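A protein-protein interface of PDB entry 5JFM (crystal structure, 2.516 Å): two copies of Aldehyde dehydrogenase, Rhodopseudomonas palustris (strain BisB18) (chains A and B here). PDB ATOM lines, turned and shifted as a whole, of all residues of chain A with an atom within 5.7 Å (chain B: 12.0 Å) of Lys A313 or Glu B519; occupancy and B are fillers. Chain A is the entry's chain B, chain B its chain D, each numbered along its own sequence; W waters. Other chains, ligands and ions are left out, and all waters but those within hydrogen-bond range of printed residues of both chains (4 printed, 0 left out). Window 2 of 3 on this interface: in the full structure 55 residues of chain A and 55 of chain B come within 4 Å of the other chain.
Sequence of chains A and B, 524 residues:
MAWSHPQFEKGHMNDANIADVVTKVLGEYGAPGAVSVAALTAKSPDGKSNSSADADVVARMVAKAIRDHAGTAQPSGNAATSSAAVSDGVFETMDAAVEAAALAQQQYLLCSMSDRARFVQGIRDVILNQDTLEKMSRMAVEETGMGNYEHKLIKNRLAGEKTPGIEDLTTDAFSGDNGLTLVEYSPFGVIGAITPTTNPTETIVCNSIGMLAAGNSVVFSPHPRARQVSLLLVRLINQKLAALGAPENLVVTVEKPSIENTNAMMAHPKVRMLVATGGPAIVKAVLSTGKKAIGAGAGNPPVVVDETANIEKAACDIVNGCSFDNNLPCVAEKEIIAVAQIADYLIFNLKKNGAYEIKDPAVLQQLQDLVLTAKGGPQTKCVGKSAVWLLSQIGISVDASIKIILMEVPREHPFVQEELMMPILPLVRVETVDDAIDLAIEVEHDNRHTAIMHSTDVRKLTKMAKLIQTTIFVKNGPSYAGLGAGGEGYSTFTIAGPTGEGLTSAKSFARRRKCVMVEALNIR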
ATOM      1  N   ASN A 310      -3.952  19.425   0.843  1.00  0.00           N
ATOM      2  CA  ASN A 310      -4.126  18.891   2.188  1.00  0.00           C
ATOM      3  C   ASN A 310      -2.776  19.003   2.904  1.00  0.00           C
ATOM      4  O   ASN A 310      -1.865  18.198   2.689  1.00  0.00           O
ATOM      5  CB  ASN A 310      -4.644  17.461   2.090  1.00  0.00           C
ATOM      6  CG  ASN A 310      -4.709  16.759   3.416  1.00  0.00           C
ATOM      7  OD1 ASN A 310      -4.380  17.316   4.466  1.00  0.00           O
ATOM      8  ND2 ASN A 310      -5.149  15.514   3.378  1.00  0.00           N
ATOM      9  N   ILE A 311      -2.642  20.020   3.751  1.00  0.00           N
ATOM     10  CA  ILE A 311      -1.353  20.358   4.344  1.00  0.00           C
ATOM     11  C   ILE A 311      -0.919  19.334   5.385  1.00  0.00           C
ATOM     12  O   ILE A 311       0.284  19.091   5.563  1.00  0.00           O
ATOM     13  CB  ILE A 311      -1.440  21.766   4.944  1.00  0.00           C
ATOM     14  CG1 ILE A 311      -1.876  22.753   3.866  1.00  0.00           C
ATOM     15  CG2 ILE A 311      -0.103  22.173   5.560  1.00  0.00           C
ATOM     16  CD1 ILE A 311      -0.819  23.020   2.834  1.00  0.00           C
ATOM     17  N   GLU A 312      -1.864  18.733   6.106  1.00  0.00           N
ATOM     18  CA  GLU A 312      -1.479  17.751   7.114  1.00  0.00           C
ATOM     19  C   GLU A 312      -0.869  16.518   6.451  1.00  0.00           C
ATOM     20  O   GLU A 312       0.091  15.926   6.963  1.00  0.00           O
ATOM     21  CB  GLU A 312      -2.692  17.369   7.971  1.00  0.00           C
ATOM     22  CG  GLU A 312      -3.365  18.519   8.753  1.00  0.00           C
ATOM     23  CD  GLU A 312      -4.386  19.332   7.934  1.00  0.00           C
ATOM     24  OE1 GLU A 312      -4.722  18.940   6.797  1.00  0.00           O
ATOM     25  OE2 GLU A 312      -4.853  20.380   8.436  1.00  0.00           O
ATOM     26  N   LYS A 313      -1.402  16.125   5.298  1.00  0.00           N
ATOM     27  CA  LYS A 313      -0.824  15.004   4.580  1.00  0.00           C
ATOM     28  C   LYS A 313       0.417  15.437   3.809  1.00  0.00           C
ATOM     29  O   LYS A 313       1.393  14.685   3.731  1.00  0.00           O
ATOM     30  CB  LYS A 313      -1.867  14.383   3.651  1.00  0.00           C
ATOM     31  CG  LYS A 313      -1.350  13.159   2.904  1.00  0.00           C
ATOM     32  CD  LYS A 313      -2.340  12.664   1.848  1.00  0.00           C
ATOM     33  CE  LYS A 313      -1.811  11.415   1.115  1.00  0.00           C
ATOM     34  NZ  LYS A 313      -0.646  11.671   0.209  1.00  0.00           N
ATOM     35  N   ALA A 314       0.414  16.652   3.259  1.00  0.00           N
ATOM     36  CA  ALA A 314       1.591  17.119   2.540  1.00  0.00           C
ATOM     37  C   ALA A 314       2.814  17.082   3.439  1.00  0.00           C
ATOM     38  O   ALA A 314       3.854  16.533   3.068  1.00  0.00           O
ATOM     39  CB  ALA A 314       1.363  18.525   1.990  1.00  0.00           C
ATOM     40  N   ALA A 315       2.693  17.627   4.650  1.00  0.00           N
ATOM     41  CA  ALA A 315       3.840  17.685   5.546  1.00  0.00           C
ATOM     42  C   ALA A 315       4.358  16.289   5.854  1.00  0.00           C
ATOM     43  O   ALA A 315       5.563  16.027   5.780  1.00  0.00           O
ATOM     44  CB  ALA A 315       3.470  18.419   6.835  1.00  0.00           C
ATOM     45  N   CYS A 316       3.452  15.376   6.189  1.00  0.00           N
ATOM     46  CA  CYS A 316       3.848  13.998   6.427  1.00  0.00           C
ATOM     47  C   CYS A 316       4.559  13.412   5.207  1.00  0.00           C
ATOM     48  O   CYS A 316       5.663  12.866   5.326  1.00  0.00           O
ATOM     49  CB  CYS A 316       2.619  13.179   6.813  1.00  0.00           C
ATOM     50  SG  CYS A 316       2.931  11.425   7.008  1.00  0.00           S
ATOM     51  N   ASP A 317       3.953  13.540   4.015  1.00  0.00           N
ATOM     52  CA  ASP A 317       4.567  12.987   2.807  1.00  0.00           C
ATOM     53  C   ASP A 317       5.914  13.638   2.514  1.00  0.00           C
ATOM     54  O   ASP A 317       6.830  12.976   2.010  1.00  0.00           O
ATOM     55  CB  ASP A 317       3.642  13.155   1.586  1.00  0.00           C
ATOM     56  CG  ASP A 317       2.302  12.417   1.730  1.00  0.00           C
ATOM     57  OD1 ASP A 317       2.215  11.467   2.534  1.00  0.00           O
ATOM     58  OD2 ASP A 317       1.328  12.800   1.033  1.00  0.00           O
ATOM     59  N   ILE A 318       6.056  14.931   2.812  1.00  0.00           N
ATOM     60  CA  ILE A 318       7.292  15.633   2.475  1.00  0.00           C
ATOM     61  C   ILE A 318       8.424  15.195   3.396  1.00  0.00           C
ATOM     62  O   ILE A 318       9.557  14.966   2.951  1.00  0.00           O
ATOM     63  CB  ILE A 318       7.068  17.155   2.525  1.00  0.00           C
ATOM     64  CG1 ILE A 318       6.153  17.584   1.377  1.00  0.00           C
ATOM     65  CG2 ILE A 318       8.384  17.895   2.450  1.00  0.00           C
ATOM     66  CD1 ILE A 318       5.835  19.053   1.369  1.00  0.00           C
ATOM     67  N   HIS A 454       2.006  19.284  -4.176  1.00  0.00           N
ATOM     68  CA  HIS A 454       0.849  19.030  -3.328  1.00  0.00           C
ATOM     69  C   HIS A 454      -0.207  20.078  -3.637  1.00  0.00           C
ATOM     70  O   HIS A 454       0.013  21.278  -3.439  1.00  0.00           O
ATOM     71  CB  HIS A 454       1.225  19.013  -1.852  1.00  0.00           C
ATOM     72  CG  HIS A 454       2.039  17.819  -1.477  1.00  0.00           C
ATOM     73  ND1 HIS A 454       1.489  16.690  -0.908  1.00  0.00           N
ATOM     74  CD2 HIS A 454       3.355  17.551  -1.652  1.00  0.00           C
ATOM     75  CE1 HIS A 454       2.439  15.792  -0.718  1.00  0.00           C
ATOM     76  NE2 HIS A 454       3.577  16.286  -1.169  1.00  0.00           N
ATOM     77  N   ASN A 476       0.574  14.752  -4.724  1.00  0.00           N
ATOM     78  CA  ASN A 476      -0.099  14.491  -3.438  1.00  0.00           C
ATOM     79  C   ASN A 476       0.369  13.190  -2.791  1.00  0.00           C
ATOM     80  O   ASN A 476      -0.428  12.439  -2.215  1.00  0.00           O
ATOM     81  CB  ASN A 476      -1.613  14.499  -3.596  1.00  0.00           C
ATOM     82  CG  ASN A 476      -2.096  15.772  -4.203  1.00  0.00           C
ATOM     83  OD1 ASN A 476      -1.657  16.852  -3.812  1.00  0.00           O
ATOM     84  ND2 ASN A 476      -2.963  15.664  -5.211  1.00  0.00           N
ATOM     85  N   GLY A 477       1.672  12.938  -2.878  1.00  0.00           N
ATOM     86  CA  GLY A 477       2.289  11.815  -2.222  1.00  0.00           C
ATOM     87  C   GLY A 477       3.771  12.054  -2.048  1.00  0.00           C
ATOM     88  O   GLY A 477       4.334  13.017  -2.586  1.00  0.00           O
ATOM     89  N   PRO A 478       4.435  11.185  -1.287  1.00  0.00           N
ATOM     90  CA  PRO A 478       5.895  11.285  -1.174  1.00  0.00           C
ATOM     91  C   PRO A 478       6.530  11.015  -2.527  1.00  0.00           C
ATOM     92  O   PRO A 478       5.975  10.292  -3.360  1.00  0.00           O
ATOM     93  CB  PRO A 478       6.256  10.197  -0.151  1.00  0.00           C
ATOM     94  CG  PRO A 478       5.124   9.220  -0.229  1.00  0.00           C
ATOM     95  CD  PRO A 478       3.896   9.971  -0.644  1.00  0.00           C
ATOM     96  N   GLY A 486       3.926   3.198  -3.080  1.00  0.00           N
ATOM     97  CA  GLY A 486       2.799   4.077  -2.841  1.00  0.00           C
ATOM     98  C   GLY A 486       2.263   4.788  -4.068  1.00  0.00           C
ATOM     99  O   GLY A 486       1.409   5.676  -3.928  1.00  0.00           O
ATOM    100  N   PHE B 174      -2.432   3.348 -15.539  1.00  0.00           N
ATOM    101  CA  PHE B 174      -2.555   2.286 -14.546  1.00  0.00           C
ATOM    102  C   PHE B 174      -3.240   2.878 -13.321  1.00  0.00           C
ATOM    103  O   PHE B 174      -2.801   3.908 -12.802  1.00  0.00           O
ATOM    104  CB  PHE B 174      -1.182   1.700 -14.207  1.00  0.00           C
ATOM    105  CG  PHE B 174      -0.319   1.468 -15.429  1.00  0.00           C
ATOM    106  CD1 PHE B 174      -0.417   0.287 -16.164  1.00  0.00           C
ATOM    107  CD2 PHE B 174       0.551   2.456 -15.881  1.00  0.00           C
ATOM    108  CE1 PHE B 174       0.345   0.086 -17.306  1.00  0.00           C
ATOM    109  CE2 PHE B 174       1.318   2.259 -17.030  1.00  0.00           C
ATOM    110  CZ  PHE B 174       1.212   1.070 -17.737  1.00  0.00           C
ATOM    111  N   SER B 175      -4.341   2.261 -12.897  1.00  0.00           N
ATOM    112  CA  SER B 175      -5.147   2.754 -11.792  1.00  0.00           C
ATOM    113  C   SER B 175      -5.365   1.642 -10.776  1.00  0.00           C
ATOM    114  O   SER B 175      -5.399   0.456 -11.125  1.00  0.00           O
ATOM    115  CB  SER B 175      -6.507   3.292 -12.260  1.00  0.00           C
ATOM    116  OG  SER B 175      -7.384   2.241 -12.623  1.00  0.00           O
ATOM    117  N   GLY B 176      -5.511   2.046  -9.522  1.00  0.00           N
ATOM    118  CA  GLY B 176      -5.574   1.091  -8.435  1.00  0.00           C
ATOM    119  C   GLY B 176      -5.666   1.808  -7.107  1.00  0.00           C
ATOM    120  O   GLY B 176      -6.037   2.976  -7.044  1.00  0.00           O
ATOM    121  N   ASP B 177      -5.315   1.089  -6.038  1.00  0.00           N
ATOM    122  CA  ASP B 177      -5.469   1.648  -4.698  1.00  0.00           C
ATOM    123  C   ASP B 177      -4.611   2.890  -4.502  1.00  0.00           C
ATOM    124  O   ASP B 177      -4.984   3.786  -3.735  1.00  0.00           O
ATOM    125  CB  ASP B 177      -5.137   0.583  -3.652  1.00  0.00           C
ATOM    126  CG  ASP B 177      -6.116  -0.598  -3.688  1.00  0.00           C
ATOM    127  OD1 ASP B 177      -7.219  -0.445  -4.261  1.00  0.00           O
ATOM    128  OD2 ASP B 177      -5.787  -1.675  -3.133  1.00  0.00           O
ATOM    129  N   ASN B 178      -3.490   2.989  -5.205  1.00  0.00           N
ATOM    130  CA  ASN B 178      -2.602   4.139  -5.084  1.00  0.00           C
ATOM    131  C   ASN B 178      -2.889   5.229  -6.107  1.00  0.00           C
ATOM    132  O   ASN B 178      -2.112   6.184  -6.215  1.00  0.00           O
ATOM    133  CB  ASN B 178      -1.144   3.689  -5.188  1.00  0.00           C
ATOM    134  CG  ASN B 178      -0.802   2.624  -4.169  1.00  0.00           C
ATOM    135  OD1 ASN B 178      -0.405   1.516  -4.518  1.00  0.00           O
ATOM    136  ND2 ASN B 178      -1.003   2.942  -2.903  1.00  0.00           N
ATOM    137  N   GLY B 179      -3.982   5.124  -6.847  1.00  0.00           N
ATOM    138  CA  GLY B 179      -4.391   6.234  -7.676  1.00  0.00           C
ATOM    139  C   GLY B 179      -4.225   5.973  -9.150  1.00  0.00           C
ATOM    140  O   GLY B 179      -4.604   4.911  -9.645  1.00  0.00           O
ATOM    141  N   LEU B 180      -3.650   6.933  -9.858  1.00  0.00           N
ATOM    142  CA  LEU B 180      -3.501   6.867 -11.301  1.00  0.00           C
ATOM    143  C   LEU B 180      -2.064   7.185 -11.665  1.00  0.00           C
ATOM    144  O   LEU B 180      -1.468   8.109 -11.107  1.00  0.00           O
ATOM    145  CB  LEU B 180      -4.434   7.861 -12.007  1.00  0.00           C
ATOM    146  CG  LEU B 180      -4.249   8.008 -13.514  1.00  0.00           C
ATOM    147  CD1 LEU B 180      -4.652   6.724 -14.207  1.00  0.00           C
ATOM    148  CD2 LEU B 180      -5.062   9.185 -14.032  1.00  0.00           C
ATOM    149  N   THR B 181      -1.510   6.412 -12.594  1.00  0.00           N
ATOM    150  CA  THR B 181      -0.216   6.708 -13.190  1.00  0.00           C
ATOM    151  C   THR B 181      -0.396   6.819 -14.699  1.00  0.00           C
ATOM    152  O   THR B 181      -0.933   5.904 -15.334  1.00  0.00           O
ATOM    153  CB  THR B 181       0.807   5.631 -12.824  1.00  0.00           C
ATOM    154  OG1 THR B 181       1.076   5.693 -11.412  1.00  0.00           O
ATOM    155  CG2 THR B 181       2.116   5.825 -13.618  1.00  0.00           C
ATOM    156  N   LEU B 182       0.015   7.953 -15.263  1.00  0.00           N
ATOM    157  CA  LEU B 182       0.001   8.171 -16.699  1.00  0.00           C
ATOM    158  C   LEU B 182       1.433   8.228 -17.197  1.00  0.00           C
ATOM    159  O   LEU B 182       2.317   8.751 -16.509  1.00  0.00           O
ATOM    160  CB  LEU B 182      -0.710   9.473 -17.071  1.00  0.00           C
ATOM    161  CG  LEU B 182      -2.163   9.659 -16.662  1.00  0.00           C
ATOM    162  CD1 LEU B 182      -2.570  11.057 -17.020  1.00  0.00           C
ATOM    163  CD2 LEU B 182      -3.048   8.659 -17.369  1.00  0.00           C
ATOM    164  N   CYS B 515       3.511  10.458 -14.934  1.00  0.00           N
ATOM    165  CA  CYS B 515       2.784  11.353 -14.035  1.00  0.00           C
ATOM    166  C   CYS B 515       1.987  10.504 -13.051  1.00  0.00           C
ATOM    167  O   CYS B 515       1.185   9.660 -13.469  1.00  0.00           O
ATOM    168  CB  CYS B 515       1.865  12.284 -14.828  1.00  0.00           C
ATOM    169  SG  CYS B 515       1.347  13.806 -14.008  1.00  0.00           S
ATOM    170  N   VAL B 516       2.209  10.715 -11.754  1.00  0.00           N
ATOM    171  CA  VAL B 516       1.647   9.853 -10.717  1.00  0.00           C
ATOM    172  C   VAL B 516       0.698  10.673  -9.850  1.00  0.00           C
ATOM    173  O   VAL B 516       1.141  11.503  -9.040  1.00  0.00           O
ATOM    174  CB  VAL B 516       2.740   9.202  -9.857  1.00  0.00           C
ATOM    175  CG1 VAL B 516       2.116   8.329  -8.777  1.00  0.00           C
ATOM    176  CG2 VAL B 516       3.691   8.401 -10.723  1.00  0.00           C
ATOM    177  N   MET B 517      -0.603  10.420  -9.995  1.00  0.00           N
ATOM    178  CA  MET B 517      -1.630  11.023  -9.148  1.00  0.00           C
ATOM    179  C   MET B 517      -1.912  10.078  -7.989  1.00  0.00           C
ATOM    180  O   MET B 517      -2.556   9.040  -8.168  1.00  0.00           O
ATOM    181  CB  MET B 517      -2.901  11.290  -9.943  1.00  0.00           C
ATOM    182  CG  MET B 517      -4.036  11.885  -9.112  1.00  0.00           C
ATOM    183  SD  MET B 517      -3.845  13.654  -8.918  1.00  0.00           S
ATOM    184  CE  MET B 517      -4.065  14.207 -10.605  1.00  0.00           C
ATOM    185  N   VAL B 518      -1.443  10.435  -6.797  1.00  0.00           N
ATOM    186  CA  VAL B 518      -1.493   9.518  -5.667  1.00  0.00           C
ATOM    187  C   VAL B 518      -2.888   9.546  -5.046  1.00  0.00           C
ATOM    188  O   VAL B 518      -3.392  10.607  -4.661  1.00  0.00           O
ATOM    189  CB  VAL B 518      -0.410   9.863  -4.637  1.00  0.00           C
ATOM    190  CG1 VAL B 518      -0.541   8.978  -3.416  1.00  0.00           C
ATOM    191  CG2 VAL B 518       0.967   9.711  -5.270  1.00  0.00           C
ATOM    192  N   GLU B 519      -3.519   8.368  -4.962  1.00  0.00           N
ATOM    193  CA  GLU B 519      -4.788   8.179  -4.248  1.00  0.00           C
ATOM    194  C   GLU B 519      -5.891   9.088  -4.792  1.00  0.00           C
ATOM    195  O   GLU B 519      -6.737   9.584  -4.049  1.00  0.00           O
ATOM    196  CB  GLU B 519      -4.609   8.379  -2.739  1.00  0.00           C
ATOM    197  CG  GLU B 519      -3.760   7.291  -2.073  1.00  0.00           C
ATOM    198  CD  GLU B 519      -3.335   7.643  -0.643  1.00  0.00           C
ATOM    199  OE1 GLU B 519      -3.909   8.586  -0.050  1.00  0.00           O
ATOM    200  OE2 GLU B 519      -2.407   6.989  -0.119  1.00  0.00           O
ATOM    201  N   ALA B 520      -5.888   9.294  -6.106  1.00  0.00           N
ATOM    202  CA  ALA B 520      -6.955  10.028  -6.772  1.00  0.00           C
ATOM    203  C   ALA B 520      -7.033   9.566  -8.223  1.00  0.00           C
ATOM    204  O   ALA B 520      -6.103   8.946  -8.752  1.00  0.00           O
ATOM    205  CB  ALA B 520      -6.741  11.545  -6.682  1.00  0.00           C
ATOM    206  N   LEU B 521      -8.174   9.854  -8.851  1.00  0.00           N
ATOM    207  CA  LEU B 521      -8.471   9.494 -10.240  1.00  0.00           C
ATOM    208  C   LEU B 521      -8.343   8.000 -10.490  1.00  0.00           C
ATOM    209  O   LEU B 521      -8.112   7.565 -11.628  1.00  0.00           O
ATOM    210  CB  LEU B 521      -7.595  10.272 -11.222  1.00  0.00           C
ATOM    211  CG  LEU B 521      -7.923  11.763 -11.269  1.00  0.00           C
ATOM    212  CD1 LEU B 521      -6.989  12.404 -12.237  1.00  0.00           C
ATOM    213  CD2 LEU B 521      -9.355  11.982 -11.698  1.00  0.00           C
ATOM    214  N   ASN B 522      -8.471   7.205  -9.431  1.00  0.00           N
ATOM    215  CA  ASN B 522      -8.689   5.772  -9.562  1.00  0.00           C
ATOM    216  C   ASN B 522     -10.200   5.564  -9.488  1.00  0.00           C
ATOM    217  O   ASN B 522     -10.769   5.239  -8.444  1.00  0.00           O
ATOM    218  CB  ASN B 522      -7.929   5.004  -8.480  1.00  0.00           C
ATOM    219  CG  ASN B 522      -8.254   5.488  -7.072  1.00  0.00           C
ATOM    220  OD1 ASN B 522      -8.625   6.641  -6.863  1.00  0.00           O
ATOM    221  ND2 ASN B 522      -8.118   4.601  -6.104  1.00  0.00           N
ATOM    222  N   ILE B 523     -10.860   5.769 -10.624  1.00  0.00           N
ATOM    223  CA  ILE B 523     -12.315   5.855 -10.646  1.00  0.00           C
ATOM    224  C   ILE B 523     -12.971   4.531 -11.017  1.00  0.00           C
ATOM    225  O   ILE B 523     -14.179   4.494 -11.245  1.00  0.00           O
ATOM    226  CB  ILE B 523     -12.788   6.985 -11.572  1.00  0.00           C
ATOM    227  CG1 ILE B 523     -12.200   6.828 -12.975  1.00  0.00           C
ATOM    228  CG2 ILE B 523     -12.388   8.327 -10.986  1.00  0.00           C
ATOM    229  CD1 ILE B 523     -13.083   6.067 -13.913  1.00  0.00           C
ATOM    230  N   ARG B 524     -12.210   3.442 -11.064  1.00  0.00           N
ATOM    231  CA  ARG B 524     -12.778   2.142 -11.387  1.00  0.00           C
ATOM    232  C   ARG B 524     -13.815   1.729 -10.346  1.00  0.00           C
ATOM    233  O   ARG B 524     -14.855   1.176 -10.701  1.00  0.00           O
ATOM    234  CB  ARG B 524     -11.683   1.077 -11.490  1.00  0.00           C
ATOM    235  CG  ARG B 524     -12.202  -0.297 -11.844  1.00  0.00           C
ATOM    236  CD  ARG B 524     -11.148  -1.385 -11.601  1.00  0.00           C
ATOM    237  NE  ARG B 524      -9.993  -1.251 -12.486  1.00  0.00           N
ATOM    238  CZ  ARG B 524      -8.785  -0.877 -12.080  1.00  0.00           C
ATOM    239  NH1 ARG B 524      -8.571  -0.610 -10.802  1.00  0.00           N
ATOM    240  NH2 ARG B 524      -7.790  -0.787 -12.951  1.00  0.00           N
HETATM  241  O   HOH W   1      -4.082  12.995  -5.736  1.00  0.00           O
HETATM  242  O   HOH W   2      -0.049   8.527   0.050  1.00  0.00           O
HETATM  243  O   HOH W   3      -3.165  11.485  -2.361  1.00  0.00           O
HETATM  244  O   HOH W   4      -0.760   5.294  -1.647  1.00  0.00           O
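Water W3 lies within hydrogen-bond range of O of Val B518 (2.5 Å) and O of Asn A476 (2.9 Å).
Water W4 lies within hydrogen-bond range of the side-chain amide nitrogen of Asn B178 (2.7 Å), the side-chain carboxylate of Glu B519 (2.8 Å) and the backbone carbonyl oxygen of Gly A486 (3.2 Å).
Water W1 lies within hydrogen-bond range of O of Val B518 (2.7 Å), ND2 of Asn A476 (2.9 Å) and SD of Met B517 (3.3 Å).
Water W2 lies within hydrogen-bond range of the side-chain carboxylate (OE2) of Glu B519 and the side-chain amino group (NZ) of Lys A313.
Of the 14 printed residues of chain A, 4 touch a printed residue of chain B.
Among the printed residues, 5 pairs touch across the chains.
No residue of chain B comes within 4 Å of Asn A310.
No residue of chain B comes within 4 Å of Ile A311.
Glu A312 touches none of the printed residues of chain B.
No residue of chain B comes within 4 Å of Ala A314.
No residue of chain B comes within 4 Å of Cys A316.
No residue of chain B comes within 4 Å of Asp A317.
Printed residues of chain B within 4 Å of Gly A486: Asn B178 (3.5 Å) and Val B518 (3.9 Å).
Of the printed residues of chain A, Asn B178 touches Gly A486 (3.5 Å).
Of the printed residues of chain A, Val B518 touches Asn A476, Gly A477 and Gly A486.
The nearest residue of chain A that does not touch Glu B519 is Gly A486 (5.5 Å).
The nearest printed residue of chain A that does not touch Val B518 is Lys A313 (4.5 Å).
No position is printed for both chains.
Of the 5 pairs that touch across the chains among the printed residues, none has its exchanged pair printed and touching as well.
The backbone carbonyl oxygen (O) of Asn A476 lies within hydrogen-bond range of the side-chain amino group (NZ) of Lys A313 (2.6 Å).
O of Asn B178 is in hydrogen-bond range of N of Glu B519 (2.9 Å).
OD2 of Asp A317 lies within salt-bridge range of NZ of Lys A313, 2.4 Å away.
OD1 of Asn A310 lies within hydrogen-bond range of N of Lys A313.
Among the printed residues, pairs that only touch across the chains: Lys A313 with Glu B519, Asn A476 with Val B518, Gly A477 with Val B518, Gly A486 with Asn B178 and Gly A486 with Val B518.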
